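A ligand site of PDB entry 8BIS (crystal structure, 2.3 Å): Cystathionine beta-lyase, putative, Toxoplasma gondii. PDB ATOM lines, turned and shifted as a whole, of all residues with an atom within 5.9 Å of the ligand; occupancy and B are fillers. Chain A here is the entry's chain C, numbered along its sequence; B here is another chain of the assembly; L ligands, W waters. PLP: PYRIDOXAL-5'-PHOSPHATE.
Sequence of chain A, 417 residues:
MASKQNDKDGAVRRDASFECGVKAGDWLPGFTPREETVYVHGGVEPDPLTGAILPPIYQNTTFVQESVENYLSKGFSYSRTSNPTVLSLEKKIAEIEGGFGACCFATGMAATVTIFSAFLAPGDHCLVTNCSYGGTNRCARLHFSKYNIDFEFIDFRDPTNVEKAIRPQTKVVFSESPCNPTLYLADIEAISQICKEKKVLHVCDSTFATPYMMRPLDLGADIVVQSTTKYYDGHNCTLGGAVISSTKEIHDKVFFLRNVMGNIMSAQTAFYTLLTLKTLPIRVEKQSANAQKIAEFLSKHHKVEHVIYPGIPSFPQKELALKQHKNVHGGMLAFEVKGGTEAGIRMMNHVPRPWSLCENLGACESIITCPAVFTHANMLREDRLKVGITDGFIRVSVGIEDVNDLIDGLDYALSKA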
ATOM      1  N   ALA A 106      -7.779 -31.907 -15.848  1.00  0.00           N
ATOM      2  CA  ALA A 106      -8.738 -30.984 -16.453  1.00  0.00           C
ATOM      3  C   ALA A 106      -8.069 -29.676 -16.875  1.00  0.00           C
ATOM      4  O   ALA A 106      -8.466 -29.093 -17.892  1.00  0.00           O
ATOM      5  CB  ALA A 106      -9.879 -30.704 -15.472  1.00  0.00           C
ATOM      6  N   THR A 107      -7.084 -29.214 -16.123  1.00  0.00           N
ATOM      7  CA  THR A 107      -6.369 -27.972 -16.416  1.00  0.00           C
ATOM      8  C   THR A 107      -4.900 -28.157 -16.045  1.00  0.00           C
ATOM      9  O   THR A 107      -4.518 -29.127 -15.403  1.00  0.00           O
ATOM     10  CB  THR A 107      -6.939 -26.785 -15.636  1.00  0.00           C
ATOM     11  OG1 THR A 107      -6.817 -27.034 -14.232  1.00  0.00           O
ATOM     12  CG2 THR A 107      -8.401 -26.526 -15.984  1.00  0.00           C
ATOM     13  N   GLY A 108      -4.081 -27.181 -16.459  1.00  0.00           N
ATOM     14  CA  GLY A 108      -2.697 -27.173 -16.000  1.00  0.00           C
ATOM     15  C   GLY A 108      -2.592 -26.848 -14.521  1.00  0.00           C
ATOM     16  O   GLY A 108      -1.747 -27.393 -13.813  1.00  0.00           O
ATOM     17  N   MET A 109      -3.454 -25.945 -14.039  1.00  0.00           N
ATOM     18  CA  MET A 109      -3.493 -25.648 -12.619  1.00  0.00           C
ATOM     19  C   MET A 109      -3.820 -26.896 -11.809  1.00  0.00           C
ATOM     20  O   MET A 109      -3.289 -27.088 -10.713  1.00  0.00           O
ATOM     21  CB  MET A 109      -4.498 -24.542 -12.329  1.00  0.00           C
ATOM     22  CG  MET A 109      -3.998 -23.139 -12.672  1.00  0.00           C
ATOM     23  SD  MET A 109      -2.430 -22.702 -11.888  1.00  0.00           S
ATOM     24  CE  MET A 109      -2.796 -23.077 -10.172  1.00  0.00           C
ATOM     25  N   ALA A 110      -4.697 -27.753 -12.335  1.00  0.00           N
ATOM     26  CA  ALA A 110      -5.005 -28.994 -11.630  1.00  0.00           C
ATOM     27  C   ALA A 110      -3.767 -29.877 -11.528  1.00  0.00           C
ATOM     28  O   ALA A 110      -3.546 -30.526 -10.499  1.00  0.00           O
ATOM     29  CB  ALA A 110      -6.141 -29.745 -12.324  1.00  0.00           C
ATOM     30  N   THR A 112      -0.538 -28.788 -11.498  1.00  0.00           N
ATOM     31  CA  THR A 112       0.333 -28.164 -10.502  1.00  0.00           C
ATOM     32  C   THR A 112      -0.172 -28.415  -9.089  1.00  0.00           C
ATOM     33  O   THR A 112       0.613 -28.742  -8.187  1.00  0.00           O
ATOM     34  CB  THR A 112       0.437 -26.665 -10.765  1.00  0.00           C
ATOM     35  OG1 THR A 112       1.004 -26.430 -12.060  1.00  0.00           O
ATOM     36  CG2 THR A 112       1.288 -25.994  -9.702  1.00  0.00           C
ATOM     37  N   TYR A 133       4.400 -18.607 -13.169  1.00  0.00           N
ATOM     38  CA  TYR A 133       3.057 -18.271 -13.615  1.00  0.00           C
ATOM     39  C   TYR A 133       2.216 -17.786 -12.439  1.00  0.00           C
ATOM     40  O   TYR A 133       2.244 -18.358 -11.354  1.00  0.00           O
ATOM     41  CB  TYR A 133       2.406 -19.506 -14.255  1.00  0.00           C
ATOM     42  CG  TYR A 133       0.944 -19.327 -14.628  1.00  0.00           C
ATOM     43  CD1 TYR A 133       0.579 -18.404 -15.596  1.00  0.00           C
ATOM     44  CD2 TYR A 133      -0.044 -20.093 -14.029  1.00  0.00           C
ATOM     45  CE1 TYR A 133      -0.754 -18.245 -15.952  1.00  0.00           C
ATOM     46  CE2 TYR A 133      -1.377 -19.933 -14.385  1.00  0.00           C
ATOM     47  CZ  TYR A 133      -1.722 -19.008 -15.340  1.00  0.00           C
ATOM     48  OH  TYR A 133      -3.035 -18.840 -15.705  1.00  0.00           O
ATOM     49  N   THR A 136       0.252 -20.323 -10.418  1.00  0.00           N
ATOM     50  CA  THR A 136       1.080 -21.154  -9.544  1.00  0.00           C
ATOM     51  C   THR A 136       1.423 -20.397  -8.258  1.00  0.00           C
ATOM     52  O   THR A 136       1.283 -20.927  -7.154  1.00  0.00           O
ATOM     53  CB  THR A 136       2.355 -21.561 -10.273  1.00  0.00           C
ATOM     54  OG1 THR A 136       2.031 -21.994 -11.601  1.00  0.00           O
ATOM     55  CG2 THR A 136       3.073 -22.672  -9.522  1.00  0.00           C
ATOM     56  N   GLU A 176      10.486 -22.922 -13.739  1.00  0.00           N
ATOM     57  CA  GLU A 176       9.681 -22.596 -14.903  1.00  0.00           C
ATOM     58  C   GLU A 176      10.607 -21.969 -15.938  1.00  0.00           C
ATOM     59  O   GLU A 176      11.422 -21.109 -15.583  1.00  0.00           O
ATOM     60  CB  GLU A 176       8.539 -21.635 -14.544  1.00  0.00           C
ATOM     61  CG  GLU A 176       7.442 -21.558 -15.579  1.00  0.00           C
ATOM     62  CD  GLU A 176       6.328 -20.618 -15.153  1.00  0.00           C
ATOM     63  OE1 GLU A 176       6.120 -19.606 -15.835  1.00  0.00           O
ATOM     64  OE2 GLU A 176       5.680 -20.902 -14.123  1.00  0.00           O
ATOM     65  N   PRO A 178      10.562 -21.134 -20.424  1.00  0.00           N
ATOM     66  CA  PRO A 178      10.609 -19.718 -20.008  1.00  0.00           C
ATOM     67  C   PRO A 178       9.442 -19.374 -19.088  1.00  0.00           C
ATOM     68  O   PRO A 178       8.394 -20.005 -19.150  1.00  0.00           O
ATOM     69  CB  PRO A 178      10.520 -18.949 -21.328  1.00  0.00           C
ATOM     70  CG  PRO A 178      10.825 -19.955 -22.400  1.00  0.00           C
ATOM     71  CD  PRO A 178      10.330 -21.264 -21.863  1.00  0.00           C
ATOM     72  N   ASN A 180       6.321 -17.356 -17.349  1.00  0.00           N
ATOM     73  CA  ASN A 180       5.177 -16.532 -17.719  1.00  0.00           C
ATOM     74  C   ASN A 180       5.125 -15.324 -16.800  1.00  0.00           C
ATOM     75  O   ASN A 180       4.986 -15.496 -15.572  1.00  0.00           O
ATOM     76  CB  ASN A 180       3.898 -17.333 -17.607  1.00  0.00           C
ATOM     77  CG  ASN A 180       2.726 -16.673 -18.306  1.00  0.00           C
ATOM     78  OD1 ASN A 180       2.727 -15.462 -18.541  1.00  0.00           O
ATOM     79  ND2 ASN A 180       1.719 -17.466 -18.658  1.00  0.00           N
ATOM     80  N   ASP A 205       7.968 -26.483 -14.999  1.00  0.00           N
ATOM     81  CA  ASP A 205       6.824 -26.093 -15.821  1.00  0.00           C
ATOM     82  C   ASP A 205       7.358 -25.600 -17.162  1.00  0.00           C
ATOM     83  O   ASP A 205       7.705 -24.426 -17.314  1.00  0.00           O
ATOM     84  CB  ASP A 205       5.997 -25.014 -15.122  1.00  0.00           C
ATOM     85  CG  ASP A 205       4.706 -24.684 -15.859  1.00  0.00           C
ATOM     86  OD1 ASP A 205       4.604 -24.952 -17.075  1.00  0.00           O
ATOM     87  OD2 ASP A 205       3.785 -24.154 -15.206  1.00  0.00           O
ATOM     88  N   THR A 207       5.659 -25.240 -19.944  1.00  0.00           N
ATOM     89  CA  THR A 207       4.528 -24.916 -20.796  1.00  0.00           C
ATOM     90  C   THR A 207       4.948 -23.987 -21.933  1.00  0.00           C
ATOM     91  O   THR A 207       4.637 -24.235 -23.102  1.00  0.00           O
ATOM     92  CB  THR A 207       3.413 -24.271 -19.972  1.00  0.00           C
ATOM     93  OG1 THR A 207       2.921 -25.219 -19.020  1.00  0.00           O
ATOM     94  CG2 THR A 207       2.283 -23.815 -20.870  1.00  0.00           C
ATOM     95  N   PHE A 208       5.653 -22.908 -21.611  1.00  0.00           N
ATOM     96  CA  PHE A 208       6.090 -21.955 -22.628  1.00  0.00           C
ATOM     97  C   PHE A 208       7.053 -22.573 -23.622  1.00  0.00           C
ATOM     98  O   PHE A 208       7.169 -22.103 -24.753  1.00  0.00           O
ATOM     99  CB  PHE A 208       6.754 -20.744 -21.958  1.00  0.00           C
ATOM    100  CG  PHE A 208       5.820 -19.606 -21.677  1.00  0.00           C
ATOM    101  CD1 PHE A 208       4.550 -19.842 -21.175  1.00  0.00           C
ATOM    102  CD2 PHE A 208       6.217 -18.299 -21.905  1.00  0.00           C
ATOM    103  CE1 PHE A 208       3.693 -18.779 -20.917  1.00  0.00           C
ATOM    104  CE2 PHE A 208       5.367 -17.243 -21.649  1.00  0.00           C
ATOM    105  CZ  PHE A 208       4.104 -17.486 -21.149  1.00  0.00           C
ATOM    106  N   SER A 227       0.821 -27.192 -19.164  1.00  0.00           N
ATOM    107  CA  SER A 227      -0.526 -26.710 -19.473  1.00  0.00           C
ATOM    108  C   SER A 227      -0.796 -27.050 -20.929  1.00  0.00           C
ATOM    109  O   SER A 227      -0.426 -26.313 -21.842  1.00  0.00           O
ATOM    110  CB  SER A 227      -0.639 -25.210 -19.207  1.00  0.00           C
ATOM    111  OG  SER A 227      -1.983 -24.803 -19.305  1.00  0.00           O
ATOM    112  N   THR A 228      -1.460 -28.189 -21.152  1.00  0.00           N
ATOM    113  CA  THR A 228      -1.791 -28.575 -22.515  1.00  0.00           C
ATOM    114  C   THR A 228      -2.776 -27.593 -23.159  1.00  0.00           C
ATOM    115  O   THR A 228      -2.938 -27.616 -24.378  1.00  0.00           O
ATOM    116  CB  THR A 228      -2.365 -29.999 -22.550  1.00  0.00           C
ATOM    117  OG1 THR A 228      -3.690 -30.009 -22.017  1.00  0.00           O
ATOM    118  CG2 THR A 228      -1.491 -30.948 -21.758  1.00  0.00           C
ATOM    119  N   THR A 229      -3.415 -26.749 -22.349  1.00  0.00           N
ATOM    120  CA  THR A 229      -4.237 -25.663 -22.884  1.00  0.00           C
ATOM    121  C   THR A 229      -3.466 -24.823 -23.891  1.00  0.00           C
ATOM    122  O   THR A 229      -4.018 -24.385 -24.907  1.00  0.00           O
ATOM    123  CB  THR A 229      -4.715 -24.783 -21.741  1.00  0.00           C
ATOM    124  OG1 THR A 229      -5.306 -25.603 -20.721  1.00  0.00           O
ATOM    125  CG2 THR A 229      -5.715 -23.761 -22.232  1.00  0.00           C
ATOM    126  N   LYS A 230      -2.179 -24.604 -23.643  1.00  0.00           N
ATOM    127  CA  LYS A 230      -1.402 -23.611 -24.355  1.00  0.00           C
ATOM    128  C   LYS A 230      -0.992 -24.062 -25.753  1.00  0.00           C
ATOM    129  O   LYS A 230      -1.596 -23.653 -26.747  1.00  0.00           O
ATOM    130  CB  LYS A 230      -0.155 -23.249 -23.544  1.00  0.00           C
ATOM    131  CG  LYS A 230      -0.327 -22.000 -22.733  1.00  0.00           C
ATOM    132  CD  LYS A 230      -1.382 -22.170 -21.663  1.00  0.00           C
ATOM    133  CE  LYS A 230      -1.637 -20.863 -20.944  1.00  0.00           C
ATOM    134  NZ  LYS A 230      -2.278 -21.079 -19.622  1.00  0.00           N
ATOM    135  N   LEU A 239      -9.071 -26.882 -22.345  1.00  0.00           N
ATOM    136  CA  LEU A 239      -8.220 -26.756 -21.170  1.00  0.00           C
ATOM    137  C   LEU A 239      -7.676 -28.130 -20.819  1.00  0.00           C
ATOM    138  O   LEU A 239      -8.382 -29.130 -20.965  1.00  0.00           O
ATOM    139  CB  LEU A 239      -8.983 -26.181 -19.980  1.00  0.00           C
ATOM    140  CG  LEU A 239      -9.750 -24.884 -20.149  1.00  0.00           C
ATOM    141  CD1 LEU A 239     -10.754 -24.741 -19.024  1.00  0.00           C
ATOM    142  CD2 LEU A 239      -8.793 -23.711 -20.163  1.00  0.00           C
ATOM    143  N   GLY A 240      -6.442 -28.179 -20.338  1.00  0.00           N
ATOM    144  CA  GLY A 240      -5.877 -29.439 -19.910  1.00  0.00           C
ATOM    145  C   GLY A 240      -4.530 -29.248 -19.262  1.00  0.00           C
ATOM    146  O   GLY A 240      -3.835 -28.250 -19.489  1.00  0.00           O
ATOM    147  N   GLY A 241      -4.154 -30.232 -18.443  1.00  0.00           N
ATOM    148  CA  GLY A 241      -2.842 -30.266 -17.843  1.00  0.00           C
ATOM    149  C   GLY A 241      -2.250 -31.640 -17.964  1.00  0.00           C
ATOM    150  O   GLY A 241      -2.934 -32.627 -18.229  1.00  0.00           O
ATOM    151  N   ASN A 360      -4.678 -16.216 -22.265  1.00  0.00           N
ATOM    152  CA  ASN A 360      -4.169 -17.442 -22.877  1.00  0.00           C
ATOM    153  C   ASN A 360      -2.990 -17.132 -23.794  1.00  0.00           C
ATOM    154  O   ASN A 360      -2.631 -15.960 -23.993  1.00  0.00           O
ATOM    155  CB  ASN A 360      -5.279 -18.176 -23.637  1.00  0.00           C
ATOM    156  CG  ASN A 360      -4.935 -19.622 -23.934  1.00  0.00           C
ATOM    157  OD1 ASN A 360      -4.147 -20.240 -23.218  1.00  0.00           O
ATOM    158  ND2 ASN A 360      -5.503 -20.162 -25.003  1.00  0.00           N
ATOM    159  N   LEU A 361      -2.383 -18.171 -24.356  1.00  0.00           N
ATOM    160  CA  LEU A 361      -1.219 -18.021 -25.229  1.00  0.00           C
ATOM    161  C   LEU A 361      -0.975 -19.348 -25.920  1.00  0.00           C
ATOM    162  O   LEU A 361      -1.595 -20.369 -25.601  1.00  0.00           O
ATOM    163  CB  LEU A 361       0.006 -17.576 -24.429  1.00  0.00           C
ATOM    164  CG  LEU A 361       0.458 -18.547 -23.339  1.00  0.00           C
ATOM    165  CD1 LEU A 361       1.724 -19.312 -23.735  1.00  0.00           C
ATOM    166  CD2 LEU A 361       0.650 -17.819 -22.034  1.00  0.00           C
ATOM    167  N   TYR B  78     -11.409 -16.379 -19.276  1.00  0.00           N
ATOM    168  CA  TYR B  78     -10.642 -17.609 -19.331  1.00  0.00           C
ATOM    169  C   TYR B  78     -11.497 -18.756 -18.809  1.00  0.00           C
ATOM    170  O   TYR B  78     -12.052 -18.658 -17.705  1.00  0.00           O
ATOM    171  CB  TYR B  78      -9.347 -17.492 -18.513  1.00  0.00           C
ATOM    172  CG  TYR B  78      -8.316 -18.549 -18.830  1.00  0.00           C
ATOM    173  CD1 TYR B  78      -7.666 -18.572 -20.054  1.00  0.00           C
ATOM    174  CD2 TYR B  78      -7.979 -19.519 -17.899  1.00  0.00           C
ATOM    175  CE1 TYR B  78      -6.710 -19.525 -20.341  1.00  0.00           C
ATOM    176  CE2 TYR B  78      -7.032 -20.485 -18.171  1.00  0.00           C
ATOM    177  CZ  TYR B  78      -6.401 -20.482 -19.402  1.00  0.00           C
ATOM    178  OH  TYR B  78      -5.457 -21.449 -19.683  1.00  0.00           O
ATOM    179  N   ARG B  80     -11.049 -21.637 -17.506  1.00  0.00           N
ATOM    180  CA  ARG B  80     -10.799 -22.263 -16.211  1.00  0.00           C
ATOM    181  C   ARG B  80     -11.505 -21.505 -15.095  1.00  0.00           C
ATOM    182  O   ARG B  80     -12.014 -22.106 -14.141  1.00  0.00           O
ATOM    183  CB  ARG B  80      -9.303 -22.348 -15.938  1.00  0.00           C
ATOM    184  CG  ARG B  80      -8.981 -22.535 -14.447  1.00  0.00           C
ATOM    185  CD  ARG B  80      -7.568 -23.047 -14.204  1.00  0.00           C
ATOM    186  NE  ARG B  80      -6.552 -22.244 -14.882  1.00  0.00           N
ATOM    187  CZ  ARG B  80      -6.158 -21.043 -14.472  1.00  0.00           C
ATOM    188  NH1 ARG B  80      -6.700 -20.484 -13.400  1.00  0.00           N
ATOM    189  NH2 ARG B  80      -5.219 -20.393 -15.147  1.00  0.00           N
ATOM    190  N   GLY B 262      -8.206 -25.376 -10.437  1.00  0.00           N
ATOM    191  CA  GLY B 262      -8.328 -25.759 -11.828  1.00  0.00           C
ATOM    192  C   GLY B 262      -9.106 -27.035 -12.079  1.00  0.00           C
ATOM    193  O   GLY B 262      -8.748 -27.804 -12.982  1.00  0.00           O
HETATM  194  N1  PLP L   1       1.761 -22.581 -16.108  1.00  0.00           N
HETATM  195  C2  PLP L   1       1.951 -21.901 -17.248  1.00  0.00           C
HETATM  196  C2A PLP L   1       3.375 -21.540 -17.641  1.00  0.00           C
HETATM  197  C3  PLP L   1       1.041 -21.618 -17.891  1.00  0.00           C
HETATM  198  O3  PLP L   1       1.275 -20.910 -19.072  1.00  0.00           O
HETATM  199  C4  PLP L   1      -0.390 -21.955 -17.552  1.00  0.00           C
HETATM  200  C4A PLP L   1      -1.482 -21.502 -18.509  1.00  0.00           C
HETATM  201  C5  PLP L   1      -0.670 -22.541 -16.593  1.00  0.00           C
HETATM  202  C6  PLP L   1       0.347 -22.948 -15.708  1.00  0.00           C
HETATM  203  C5A PLP L   1      -2.101 -22.881 -16.199  1.00  0.00           C
HETATM  204  O4P PLP L   1      -2.634 -23.934 -16.948  1.00  0.00           O
HETATM  205  P   PLP L   1      -4.263 -23.898 -17.120  1.00  0.00           P
HETATM  206  O1P PLP L   1      -4.901 -24.229 -15.798  1.00  0.00           O
HETATM  207  O2P PLP L   1      -4.683 -22.514 -17.521  1.00  0.00           O
HETATM  208  O3P PLP L   1      -4.656 -24.910 -18.166  1.00  0.00           O
HETATM  209  O   HOH W   1       0.664 -24.109 -12.634  1.00  0.00           O
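C4A of the ligand is covalently linked to NZ of Lys 230 (1.4 Å). O4P of the ligand sits at hydrogen-bond distance from OG of Ser 227, at 2.6 Å. An oxygen (O3P) of the ligand sits at hydrogen-bond distance from the backbone NH (N) of Gly 108, 2.9 Å away. The guanidinium group (NE) of Arg 80 of chain B lies within salt-bridge range of an oxygen (O1P) of the ligand. An oxygen (O3) of the ligand is in hydrogen-bond range of the side-chain amide nitrogen (ND2) of Asn 180, at 3.5 Å. OH of Tyr 78 of chain B is in hydrogen-bond range of O2P of the ligand. O3P of the ligand is in hydrogen-bond range of OG1 of Thr 229 (2.7 Å). The side-chain carboxylate (OD2) of Asp 205 lies within hydrogen-bond range of a nitrogen (N1) of the ligand, at 2.7 Å. O1P of the ligand lies within hydrogen-bond range of N of Met 109 (2.9 Å).
CB of Thr 107 touches O1P of the ligand, at 3.3 Å. CD2 of Tyr 133 touches C6 of the ligand, at 3.3 Å. OE1 of Glu 176 touches C2A of the ligand, at 3.8 Å. Thr 207 touches the ligand. Phe 208 touches the ligand. O of Gly 240 touches O3P of the ligand, 3.7 Å away. Within 4 Å of the ligand: Thr 107, Gly 108, Met 109, Tyr 133, Glu 176, Asn 180, Asp 205, Thr 207, Phe 208, Ser 227, Thr 229, Lys 230, Gly 240, Tyr 78 of chain B and Arg 80 of chain B. The nearest printed residue that does not touch the ligand is Leu 361 (4.3 Å).
OG1 of Thr 112 sits at hydrogen-bond distance from O of Gly 108 (3.4 Å). The backbone NH (N) of Gly 241 lies close to the backbone carbonyl oxygen (O) of Thr 107, at 3.3 Å. The side-chain hydroxyl (OG1) of Thr 229 is in hydrogen-bond range of the backbone NH (N) of Gly 240 (2.8 Å). The backbone NH of Gly 240 lies close to the backbone carbonyl oxygen of Ala 106, at 3.3 Å. OE1 of Glu 176 is in hydrogen-bond range of N of Asn 180, at 2.7 Å. The side-chain carboxylate (OD1) of Asp 205 is in hydrogen-bond range of the side-chain hydroxyl (OG1) of Thr 207, at 2.6 Å. The side-chain amino group (NZ) of Lys 230 lies within hydrogen-bond range of the side-chain hydroxyl (OH) of Tyr 78 of chain B (3.2 Å). N of Ser 227 is in hydrogen-bond range of OG1 of Thr 207 (2.9 Å).
Water W1 lies within hydrogen-bond range of the side-chain hydroxyl (OG1) of Thr 112 (2.4 Å), the side-chain hydroxyl (OG1) of Thr 136 (2.7 Å) and the side-chain sulfur (SD) of Met 109 (3.5 Å).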
